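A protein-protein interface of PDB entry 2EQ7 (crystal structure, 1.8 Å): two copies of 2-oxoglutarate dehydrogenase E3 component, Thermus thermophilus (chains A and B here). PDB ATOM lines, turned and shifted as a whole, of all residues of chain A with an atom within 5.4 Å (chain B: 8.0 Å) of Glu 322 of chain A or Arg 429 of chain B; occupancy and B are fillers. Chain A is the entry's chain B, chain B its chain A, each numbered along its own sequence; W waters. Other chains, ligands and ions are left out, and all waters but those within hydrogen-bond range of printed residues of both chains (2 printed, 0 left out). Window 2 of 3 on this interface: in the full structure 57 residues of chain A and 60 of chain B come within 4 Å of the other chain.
The side-chain carboxylate (OE2) of Glu 322 of chain A lies within salt-bridge range of the guanidinium group (NH2) of Arg 429 of chain B.
The side-chain amino group (NZ) of Lys 442 of chain B is in salt-bridge range of the side-chain carboxylate (OE1) of Glu 315 of chain A.
The side-chain hydroxyl of Ser 423 of chain B is in hydrogen-bond range of the side-chain carboxylate of Asp 426 of chain B (2.9 Å).
The backbone carbonyl oxygen of Gly 428 of chain B lies within hydrogen-bond range of the side-chain amino group of Lys 442 of chain B (2.6 Å).
The backbone carbonyl oxygen (O) of Ala 430 of chain B sits at hydrogen-bond distance from a ring nitrogen (ND1) of His 432 of chain B, 2.7 Å away.
The side-chain amino group of Lys 442 of chain B is in hydrogen-bond range of the backbone carbonyl oxygen of Ala 430 of chain B.
The guanidinium group (NE) of Arg 19 of chain A is in salt-bridge range of the side-chain carboxylate (OE1) of Glu 322 of chain A.
N of Gly 327 of chain A is in hydrogen-bond range of O of Glu 322 of chain A.
Glu 315 of chain A touches Ala 430 of chain B (OE1 to O, 3.96 Å).
Glu 315 of chain A touches Pro 431 of chain B (OE1 to CA, 3.8 Å).
CG2 of Ile 318 of chain A touches NH2 of Arg 429 of chain B, 3.8 Å away.
Phe 419 of chain A touches Asp 426 of chain B.
Phe 419 of chain A touches Arg 429 of chain B.
Phe 419 of chain A touches Ala 430 of chain B (CD2 to CB, 3.4 Å).
CD of Pro 431 of chain B touches CD1 of Phe 419 of chain A, 3.6 Å away.
Of the printed residues of chain A, Arg 429 of chain B touches Ile 318, Glu 322 and Phe 419.
Printed residues of chain A within 4 Å of Asp 426 of chain B: Phe 419.
Of the printed residues of chain B, Ile 318 of chain A touches Arg 429 (3.8 Å).
Of the printed residues of chain A, Ala 430 of chain B touches Glu 315 (3.96 Å) and Phe 419 (3.4 Å).
Printed residues of chain B within 4 Å of Phe 419 of chain A: Asp 426, Arg 429, Ala 430 and Pro 431.
Of the printed residues of chain B, Glu 315 of chain A touches Ala 430 (3.96 Å), Pro 431 (3.8 Å) and Lys 442 (3.5 Å).
Ala 424 of chain B touches none of the printed residues of chain A.
The nearest residue of chain B that does not touch Glu 322 of chain A is Trp 449 of chain B (5.9 Å).
The nearest printed residue of chain B that does not touch Phe 419 of chain A is Leu 427 of chain B (5.6 Å).
Among the printed residues, 9 pairs touch across the chains.
Among the printed residues, Asp or Glu carboxylates within 4 Å of a Lys or Arg side-chain nitrogen of the other chain: Glu 315 of chain A with Lys 442 of chain B (3.5 Å) and Glu 322 of chain A with Arg 429 of chain B (2.5 Å).
No position is printed for both chains.
Water W2 lies within hydrogen-bond range of the side-chain carboxylate of Glu 315 of chain A, the backbone NH of His 432 of chain B and the side-chain amino group of Lys 442 of chain B.
Water W1 lies within hydrogen-bond range of the side-chain carboxylate (OE2) of Glu 322 of chain A (2.8 Å) and the guanidinium group (NH2) of Arg 429 of chain B (3.2 Å).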
ATOM      1  N   ARG A  19      18.978  18.731 -11.548  1.00  0.00           N
ATOM      2  CA  ARG A  19      19.245  20.142 -11.813  1.00  0.00           C
ATOM      3  C   ARG A  19      20.114  20.729 -10.703  1.00  0.00           C
ATOM      4  O   ARG A  19      21.016  21.530 -10.962  1.00  0.00           O
ATOM      5  CB  ARG A  19      17.933  20.926 -11.920  1.00  0.00           C
ATOM      6  CG  ARG A  19      18.103  22.405 -12.261  1.00  0.00           C
ATOM      7  CD  ARG A  19      18.914  22.609 -13.544  1.00  0.00           C
ATOM      8  NE  ARG A  19      19.086  24.025 -13.865  1.00  0.00           N
ATOM      9  CZ  ARG A  19      20.078  24.509 -14.609  1.00  0.00           C
ATOM     10  NH1 ARG A  19      20.995  23.689 -15.110  1.00  0.00           N
ATOM     11  NH2 ARG A  19      20.157  25.811 -14.852  1.00  0.00           N
ATOM     12  N   LEU A  23      23.967  22.388 -10.911  1.00  0.00           N
ATOM     13  CA  LEU A  23      24.266  23.710 -10.380  1.00  0.00           C
ATOM     14  C   LEU A  23      25.364  23.681  -9.317  1.00  0.00           C
ATOM     15  O   LEU A  23      25.707  24.717  -8.743  1.00  0.00           O
ATOM     16  CB  LEU A  23      22.992  24.350  -9.817  1.00  0.00           C
ATOM     17  CG  LEU A  23      21.907  24.653 -10.857  1.00  0.00           C
ATOM     18  CD1 LEU A  23      20.669  25.205 -10.168  1.00  0.00           C
ATOM     19  CD2 LEU A  23      22.439  25.651 -11.877  1.00  0.00           C
ATOM     20  N   GLU A 315       9.083  20.923 -13.698  1.00  0.00           N
ATOM     21  CA  GLU A 315       9.353  22.341 -13.903  1.00  0.00           C
ATOM     22  C   GLU A 315       9.442  23.078 -12.569  1.00  0.00           C
ATOM     23  O   GLU A 315      10.254  23.994 -12.409  1.00  0.00           O
ATOM     24  CB  GLU A 315       8.268  22.977 -14.780  1.00  0.00           C
ATOM     25  CG  GLU A 315       8.318  22.544 -16.245  1.00  0.00           C
ATOM     26  CD  GLU A 315       9.620  22.931 -16.935  1.00  0.00           C
ATOM     27  OE1 GLU A 315       9.804  22.555 -18.113  1.00  0.00           O
ATOM     28  OE2 GLU A 315      10.457  23.615 -16.308  1.00  0.00           O
ATOM     29  N   GLY A 317      10.387  21.695  -9.784  1.00  0.00           N
ATOM     30  CA  GLY A 317      11.614  21.240  -9.158  1.00  0.00           C
ATOM     31  C   GLY A 317      12.785  22.073  -9.648  1.00  0.00           C
ATOM     32  O   GLY A 317      13.646  22.485  -8.862  1.00  0.00           O
ATOM     33  N   ILE A 318      12.819  22.322 -10.955  1.00  0.00           N
ATOM     34  CA  ILE A 318      13.883  23.121 -11.555  1.00  0.00           C
ATOM     35  C   ILE A 318      13.842  24.547 -11.008  1.00  0.00           C
ATOM     36  O   ILE A 318      14.870  25.105 -10.615  1.00  0.00           O
ATOM     37  CB  ILE A 318      13.743  23.150 -13.102  1.00  0.00           C
ATOM     38  CG1 ILE A 318      14.101  21.774 -13.673  1.00  0.00           C
ATOM     39  CG2 ILE A 318      14.632  24.236 -13.702  1.00  0.00           C
ATOM     40  CD1 ILE A 318      13.836  21.636 -15.167  1.00  0.00           C
ATOM     41  N   ALA A 319      12.647  25.128 -10.969  1.00  0.00           N
ATOM     42  CA  ALA A 319      12.480  26.488 -10.469  1.00  0.00           C
ATOM     43  C   ALA A 319      12.861  26.600  -8.995  1.00  0.00           C
ATOM     44  O   ALA A 319      13.437  27.606  -8.571  1.00  0.00           O
ATOM     45  CB  ALA A 319      11.045  26.948 -10.671  1.00  0.00           C
ATOM     46  N   ALA A 320      12.543  25.573  -8.212  1.00  0.00           N
ATOM     47  CA  ALA A 320      12.867  25.588  -6.786  1.00  0.00           C
ATOM     48  C   ALA A 320      14.375  25.613  -6.544  1.00  0.00           C
ATOM     49  O   ALA A 320      14.879  26.450  -5.790  1.00  0.00           O
ATOM     50  CB  ALA A 320      12.252  24.376  -6.091  1.00  0.00           C
ATOM     51  N   VAL A 321      15.099  24.701  -7.181  1.00  0.00           N
ATOM     52  CA  VAL A 321      16.541  24.644  -6.989  1.00  0.00           C
ATOM     53  C   VAL A 321      17.252  25.858  -7.576  1.00  0.00           C
ATOM     54  O   VAL A 321      18.225  26.343  -7.004  1.00  0.00           O
ATOM     55  CB  VAL A 321      17.145  23.353  -7.586  1.00  0.00           C
ATOM     56  CG1 VAL A 321      16.521  22.139  -6.912  1.00  0.00           C
ATOM     57  CG2 VAL A 321      16.922  23.309  -9.084  1.00  0.00           C
ATOM     58  N   GLU A 322      16.774  26.355  -8.712  1.00  0.00           N
ATOM     59  CA  GLU A 322      17.403  27.523  -9.307  1.00  0.00           C
ATOM     60  C   GLU A 322      17.220  28.726  -8.391  1.00  0.00           C
ATOM     61  O   GLU A 322      18.081  29.606  -8.329  1.00  0.00           O
ATOM     62  CB  GLU A 322      16.827  27.794 -10.699  1.00  0.00           C
ATOM     63  CG  GLU A 322      17.302  26.774 -11.727  1.00  0.00           C
ATOM     64  CD  GLU A 322      16.899  27.114 -13.144  1.00  0.00           C
ATOM     65  OE1 GLU A 322      17.355  26.409 -14.069  1.00  0.00           O
ATOM     66  OE2 GLU A 322      16.126  28.073 -13.336  1.00  0.00           O
ATOM     67  N   HIS A 323      16.107  28.762  -7.663  1.00  0.00           N
ATOM     68  CA  HIS A 323      15.883  29.867  -6.738  1.00  0.00           C
ATOM     69  C   HIS A 323      16.856  29.724  -5.569  1.00  0.00           C
ATOM     70  O   HIS A 323      17.383  30.715  -5.065  1.00  0.00           O
ATOM     71  CB  HIS A 323      14.452  29.865  -6.198  1.00  0.00           C
ATOM     72  CG  HIS A 323      14.186  30.969  -5.224  1.00  0.00           C
ATOM     73  ND1 HIS A 323      14.001  32.278  -5.613  1.00  0.00           N
ATOM     74  CD2 HIS A 323      14.135  30.968  -3.871  1.00  0.00           C
ATOM     75  CE1 HIS A 323      13.847  33.037  -4.541  1.00  0.00           C
ATOM     76  NE2 HIS A 323      13.924  32.265  -3.472  1.00  0.00           N
ATOM     77  N   MET A 324      17.085  28.484  -5.144  1.00  0.00           N
ATOM     78  CA  MET A 324      17.998  28.196  -4.037  1.00  0.00           C
ATOM     79  C   MET A 324      19.411  28.668  -4.342  1.00  0.00           C
ATOM     80  O   MET A 324      20.093  29.225  -3.482  1.00  0.00           O
ATOM     81  CB  MET A 324      18.066  26.693  -3.766  1.00  0.00           C
ATOM     82  CG  MET A 324      16.805  26.062  -3.219  1.00  0.00           C
ATOM     83  SD  MET A 324      16.990  24.274  -3.205  1.00  0.00           S
ATOM     84  CE  MET A 324      15.248  23.755  -3.083  1.00  0.00           C
ATOM     85  N   VAL A 325      19.844  28.426  -5.573  1.00  0.00           N
ATOM     86  CA  VAL A 325      21.193  28.774  -6.001  1.00  0.00           C
ATOM     87  C   VAL A 325      21.369  30.175  -6.580  1.00  0.00           C
ATOM     88  O   VAL A 325      22.366  30.840  -6.301  1.00  0.00           O
ATOM     89  CB  VAL A 325      21.706  27.761  -7.050  1.00  0.00           C
ATOM     90  CG1 VAL A 325      23.148  28.076  -7.420  1.00  0.00           C
ATOM     91  CG2 VAL A 325      21.583  26.342  -6.507  1.00  0.00           C
ATOM     92  N   ARG A 326      20.405  30.619  -7.381  1.00  0.00           N
ATOM     93  CA  ARG A 326      20.493  31.926  -8.024  1.00  0.00           C
ATOM     94  C   ARG A 326      19.553  32.998  -7.485  1.00  0.00           C
ATOM     95  O   ARG A 326      19.713  34.178  -7.800  1.00  0.00           O
ATOM     96  CB  ARG A 326      20.272  31.759  -9.528  1.00  0.00           C
ATOM     97  CG  ARG A 326      21.297  30.851 -10.185  1.00  0.00           C
ATOM     98  CD  ARG A 326      20.919  30.508 -11.612  1.00  0.00           C
ATOM     99  NE  ARG A 326      21.968  29.739 -12.277  1.00  0.00           N
ATOM    100  CZ  ARG A 326      21.845  29.193 -13.483  1.00  0.00           C
ATOM    101  NH1 ARG A 326      20.712  29.326 -14.161  1.00  0.00           N
ATOM    102  NH2 ARG A 326      22.859  28.520 -14.014  1.00  0.00           N
ATOM    103  N   GLY A 327      18.578  32.595  -6.679  1.00  0.00           N
ATOM    104  CA  GLY A 327      17.640  33.556  -6.122  1.00  0.00           C
ATOM    105  C   GLY A 327      16.566  33.987  -7.103  1.00  0.00           C
ATOM    106  O   GLY A 327      15.870  34.979  -6.880  1.00  0.00           O
ATOM    107  N   PHE A 328      16.436  33.236  -8.194  1.00  0.00           N
ATOM    108  CA  PHE A 328      15.448  33.521  -9.231  1.00  0.00           C
ATOM    109  C   PHE A 328      14.486  32.341  -9.347  1.00  0.00           C
ATOM    110  O   PHE A 328      14.018  31.816  -8.338  1.00  0.00           O
ATOM    111  CB  PHE A 328      16.153  33.750 -10.572  1.00  0.00           C
ATOM    112  CG  PHE A 328      17.070  34.943 -10.587  1.00  0.00           C
ATOM    113  CD1 PHE A 328      18.106  35.023 -11.514  1.00  0.00           C
ATOM    114  CD2 PHE A 328      16.891  35.996  -9.691  1.00  0.00           C
ATOM    115  CE1 PHE A 328      18.948  36.133 -11.552  1.00  0.00           C
ATOM    116  CE2 PHE A 328      17.728  37.111  -9.720  1.00  0.00           C
ATOM    117  CZ  PHE A 328      18.759  37.180 -10.652  1.00  0.00           C
ATOM    118  N   GLY A 329      14.192  31.927 -10.573  1.00  0.00           N
ATOM    119  CA  GLY A 329      13.298  30.799 -10.771  1.00  0.00           C
ATOM    120  C   GLY A 329      11.890  31.194 -11.164  1.00  0.00           C
ATOM    121  O   GLY A 329      11.299  32.103 -10.582  1.00  0.00           O
ATOM    122  N   PHE A 419       4.808  29.991 -24.475  1.00  0.00           N
ATOM    123  CA  PHE A 419       6.039  30.246 -23.735  1.00  0.00           C
ATOM    124  C   PHE A 419       6.707  31.514 -24.261  1.00  0.00           C
ATOM    125  O   PHE A 419       7.309  32.273 -23.497  1.00  0.00           O
ATOM    126  CB  PHE A 419       6.998  29.061 -23.883  1.00  0.00           C
ATOM    127  CG  PHE A 419       8.182  29.114 -22.955  1.00  0.00           C
ATOM    128  CD1 PHE A 419       7.999  29.162 -21.575  1.00  0.00           C
ATOM    129  CD2 PHE A 419       9.480  29.091 -23.458  1.00  0.00           C
ATOM    130  CE1 PHE A 419       9.092  29.184 -20.708  1.00  0.00           C
ATOM    131  CE2 PHE A 419      10.585  29.113 -22.596  1.00  0.00           C
ATOM    132  CZ  PHE A 419      10.388  29.160 -21.220  1.00  0.00           C
ATOM    133  N   SER B 423      16.836  30.575 -29.054  1.00  0.00           N
ATOM    134  CA  SER B 423      18.125  29.997 -28.710  1.00  0.00           C
ATOM    135  C   SER B 423      17.843  28.579 -28.236  1.00  0.00           C
ATOM    136  O   SER B 423      16.688  28.230 -27.976  1.00  0.00           O
ATOM    137  CB  SER B 423      18.786  30.788 -27.575  1.00  0.00           C
ATOM    138  OG  SER B 423      18.010  30.709 -26.388  1.00  0.00           O
ATOM    139  N   ALA B 424      18.887  27.764 -28.127  1.00  0.00           N
ATOM    140  CA  ALA B 424      18.727  26.396 -27.661  1.00  0.00           C
ATOM    141  C   ALA B 424      18.159  26.438 -26.244  1.00  0.00           C
ATOM    142  O   ALA B 424      17.338  25.600 -25.867  1.00  0.00           O
ATOM    143  CB  ALA B 424      20.060  25.677 -27.676  1.00  0.00           C
ATOM    144  N   GLU B 425      18.588  27.428 -25.464  1.00  0.00           N
ATOM    145  CA  GLU B 425      18.101  27.574 -24.095  1.00  0.00           C
ATOM    146  C   GLU B 425      16.590  27.794 -24.076  1.00  0.00           C
ATOM    147  O   GLU B 425      15.878  27.170 -23.290  1.00  0.00           O
ATOM    148  CB  GLU B 425      18.787  28.752 -23.397  1.00  0.00           C
ATOM    149  CG  GLU B 425      18.439  28.864 -21.919  1.00  0.00           C
ATOM    150  CD  GLU B 425      18.969  30.137 -21.280  1.00  0.00           C
ATOM    151  OE1 GLU B 425      19.926  30.725 -21.824  1.00  0.00           O
ATOM    152  OE2 GLU B 425      18.433  30.540 -20.225  1.00  0.00           O
ATOM    153  N   ASP B 426      16.110  28.689 -24.938  1.00  0.00           N
ATOM    154  CA  ASP B 426      14.685  29.004 -25.035  1.00  0.00           C
ATOM    155  C   ASP B 426      13.848  27.750 -25.263  1.00  0.00           C
ATOM    156  O   ASP B 426      12.849  27.522 -24.576  1.00  0.00           O
ATOM    157  CB  ASP B 426      14.432  29.975 -26.192  1.00  0.00           C
ATOM    158  CG  ASP B 426      14.956  31.368 -25.918  1.00  0.00           C
ATOM    159  OD1 ASP B 426      15.459  32.006 -26.866  1.00  0.00           O
ATOM    160  OD2 ASP B 426      14.852  31.831 -24.766  1.00  0.00           O
ATOM    161  N   LEU B 427      14.253  26.954 -26.249  1.00  0.00           N
ATOM    162  CA  LEU B 427      13.548  25.722 -26.583  1.00  0.00           C
ATOM    163  C   LEU B 427      13.653  24.705 -25.451  1.00  0.00           C
ATOM    164  O   LEU B 427      12.653  24.114 -25.044  1.00  0.00           O
ATOM    165  CB  LEU B 427      14.121  25.127 -27.881  1.00  0.00           C
ATOM    166  CG  LEU B 427      13.525  23.813 -28.400  1.00  0.00           C
ATOM    167  CD1 LEU B 427      12.005  23.904 -28.422  1.00  0.00           C
ATOM    168  CD2 LEU B 427      14.062  23.526 -29.800  1.00  0.00           C
ATOM    169  N   GLY B 428      14.865  24.518 -24.938  1.00  0.00           N
ATOM    170  CA  GLY B 428      15.080  23.564 -23.867  1.00  0.00           C
ATOM    171  C   GLY B 428      14.359  23.866 -22.566  1.00  0.00           C
ATOM    172  O   GLY B 428      14.021  22.947 -21.820  1.00  0.00           O
ATOM    173  N   ARG B 429      14.119  25.142 -22.285  1.00  0.00           N
ATOM    174  CA  ARG B 429      13.447  25.518 -21.048  1.00  0.00           C
ATOM    175  C   ARG B 429      11.928  25.584 -21.160  1.00  0.00           C
ATOM    176  O   ARG B 429      11.232  25.691 -20.152  1.00  0.00           O
ATOM    177  CB  ARG B 429      13.985  26.859 -20.540  1.00  0.00           C
ATOM    178  CG  ARG B 429      15.488  26.864 -20.327  1.00  0.00           C
ATOM    179  CD  ARG B 429      15.903  27.829 -19.231  1.00  0.00           C
ATOM    180  NE  ARG B 429      15.383  27.407 -17.932  1.00  0.00           N
ATOM    181  CZ  ARG B 429      15.785  27.901 -16.766  1.00  0.00           C
ATOM    182  NH1 ARG B 429      16.721  28.840 -16.723  1.00  0.00           N
ATOM    183  NH2 ARG B 429      15.251  27.452 -15.639  1.00  0.00           N
ATOM    184  N   ALA B 430      11.411  25.520 -22.382  1.00  0.00           N
ATOM    185  CA  ALA B 430       9.968  25.575 -22.581  1.00  0.00           C
ATOM    186  C   ALA B 430       9.315  24.316 -22.017  1.00  0.00           C
ATOM    187  O   ALA B 430       9.914  23.238 -22.016  1.00  0.00           O
ATOM    188  CB  ALA B 430       9.643  25.715 -24.069  1.00  0.00           C
ATOM    189  N   PRO B 431       8.077  24.439 -21.517  1.00  0.00           N
ATOM    190  CA  PRO B 431       7.397  23.266 -20.963  1.00  0.00           C
ATOM    191  C   PRO B 431       7.085  22.257 -22.066  1.00  0.00           C
ATOM    192  O   PRO B 431       6.689  22.639 -23.168  1.00  0.00           O
ATOM    193  CB  PRO B 431       6.114  23.853 -20.368  1.00  0.00           C
ATOM    194  CG  PRO B 431       6.473  25.288 -20.093  1.00  0.00           C
ATOM    195  CD  PRO B 431       7.273  25.653 -21.313  1.00  0.00           C
ATOM    196  N   HIS B 432       7.288  20.978 -21.768  1.00  0.00           N
ATOM    197  CA  HIS B 432       6.983  19.905 -22.709  1.00  0.00           C
ATOM    198  C   HIS B 432       6.246  18.808 -21.954  1.00  0.00           C
ATOM    199  O   HIS B 432       6.636  18.435 -20.845  1.00  0.00           O
ATOM    200  CB  HIS B 432       8.254  19.338 -23.341  1.00  0.00           C
ATOM    201  CG  HIS B 432       8.904  20.270 -24.311  1.00  0.00           C
ATOM    202  ND1 HIS B 432       9.669  21.344 -23.913  1.00  0.00           N
ATOM    203  CD2 HIS B 432       8.866  20.313 -25.665  1.00  0.00           C
ATOM    204  CE1 HIS B 432      10.074  22.011 -24.980  1.00  0.00           C
ATOM    205  NE2 HIS B 432       9.600  21.408 -26.055  1.00  0.00           N
ATOM    206  N   LYS B 442      13.329  18.692 -26.717  1.00  0.00           N
ATOM    207  CA  LYS B 442      13.664  19.506 -25.555  1.00  0.00           C
ATOM    208  C   LYS B 442      15.047  19.120 -25.034  1.00  0.00           C
ATOM    209  O   LYS B 442      15.887  19.982 -24.780  1.00  0.00           O
ATOM    210  CB  LYS B 442      12.626  19.302 -24.443  1.00  0.00           C
ATOM    211  CG  LYS B 442      12.939  20.037 -23.139  1.00  0.00           C
ATOM    212  CD  LYS B 442      12.032  19.563 -22.009  1.00  0.00           C
ATOM    213  CE  LYS B 442      12.341  20.259 -20.686  1.00  0.00           C
ATOM    214  NZ  LYS B 442      11.993  21.713 -20.690  1.00  0.00           N
ATOM    215  N   GLU B 443      15.288  17.820 -24.879  1.00  0.00           N
ATOM    216  CA  GLU B 443      16.576  17.347 -24.378  1.00  0.00           C
ATOM    217  C   GLU B 443      17.721  17.640 -25.341  1.00  0.00           C
ATOM    218  O   GLU B 443      18.849  17.897 -24.916  1.00  0.00           O
ATOM    219  CB  GLU B 443      16.515  15.845 -24.086  1.00  0.00           C
ATOM    220  CG  GLU B 443      15.700  15.480 -22.849  1.00  0.00           C
ATOM    221  CD  GLU B 443      16.326  15.993 -21.558  1.00  0.00           C
ATOM    222  OE1 GLU B 443      17.532  15.752 -21.346  1.00  0.00           O
ATOM    223  OE2 GLU B 443      15.612  16.628 -20.753  1.00  0.00           O
ATOM    224  N   ALA B 445      17.864  20.206 -27.295  1.00  0.00           N
ATOM    225  CA  ALA B 445      18.081  21.642 -27.148  1.00  0.00           C
ATOM    226  C   ALA B 445      18.914  21.933 -25.899  1.00  0.00           C
ATOM    227  O   ALA B 445      19.864  22.715 -25.945  1.00  0.00           O
ATOM    228  CB  ALA B 445      16.740  22.364 -27.068  1.00  0.00           C
ATOM    229  N   LEU B 446      18.553  21.305 -24.783  1.00  0.00           N
ATOM    230  CA  LEU B 446      19.292  21.496 -23.537  1.00  0.00           C
ATOM    231  C   LEU B 446      20.744  21.061 -23.711  1.00  0.00           C
ATOM    232  O   LEU B 446      21.665  21.736 -23.241  1.00  0.00           O
ATOM    233  CB  LEU B 446      18.657  20.684 -22.400  1.00  0.00           C
ATOM    234  CG  LEU B 446      17.300  21.150 -21.864  1.00  0.00           C
ATOM    235  CD1 LEU B 446      16.815  20.172 -20.802  1.00  0.00           C
ATOM    236  CD2 LEU B 446      17.426  22.557 -21.276  1.00  0.00           C
ATOM    237  N   TRP B 449      22.556  23.721 -25.740  1.00  0.00           N
ATOM    238  CA  TRP B 449      22.761  24.904 -24.921  1.00  0.00           C
ATOM    239  C   TRP B 449      23.867  24.668 -23.899  1.00  0.00           C
ATOM    240  O   TRP B 449      24.728  25.521 -23.698  1.00  0.00           O
ATOM    241  CB  TRP B 449      21.453  25.274 -24.210  1.00  0.00           C
ATOM    242  CG  TRP B 449      21.587  26.328 -23.141  1.00  0.00           C
ATOM    243  CD1 TRP B 449      22.270  27.507 -23.228  1.00  0.00           C
ATOM    244  CD2 TRP B 449      21.002  26.300 -21.832  1.00  0.00           C
ATOM    245  NE1 TRP B 449      22.148  28.217 -22.055  1.00  0.00           N
ATOM    246  CE2 TRP B 449      21.375  27.498 -21.181  1.00  0.00           C
ATOM    247  CE3 TRP B 449      20.199  25.378 -21.146  1.00  0.00           C
ATOM    248  CZ2 TRP B 449      20.971  27.799 -19.874  1.00  0.00           C
ATOM    249  CZ3 TRP B 449      19.796  25.676 -19.845  1.00  0.00           C
ATOM    250  CH2 TRP B 449      20.185  26.879 -19.224  1.00  0.00           C
ATOM    251  N   GLU B 450      23.847  23.493 -23.277  1.00  0.00           N
ATOM    252  CA  GLU B 450      24.825  23.144 -22.256  1.00  0.00           C
ATOM    253  C   GLU B 450      26.139  22.565 -22.779  1.00  0.00           C
ATOM    254  O   GLU B 450      26.923  22.006 -22.014  1.00  0.00           O
ATOM    255  CB  GLU B 450      24.178  22.187 -21.253  1.00  0.00           C
ATOM    256  CG  GLU B 450      22.993  22.818 -20.534  1.00  0.00           C
ATOM    257  CD  GLU B 450      22.161  21.821 -19.754  1.00  0.00           C
ATOM    258  OE1 GLU B 450      21.203  22.255 -19.079  1.00  0.00           O
ATOM    259  OE2 GLU B 450      22.456  20.608 -19.821  1.00  0.00           O
HETATM  260  O   HOH W   1      13.302  28.373 -13.234  1.00  0.00           O
HETATM  261  O   HOH W   2       9.214  20.378 -19.483  1.00  0.00           O
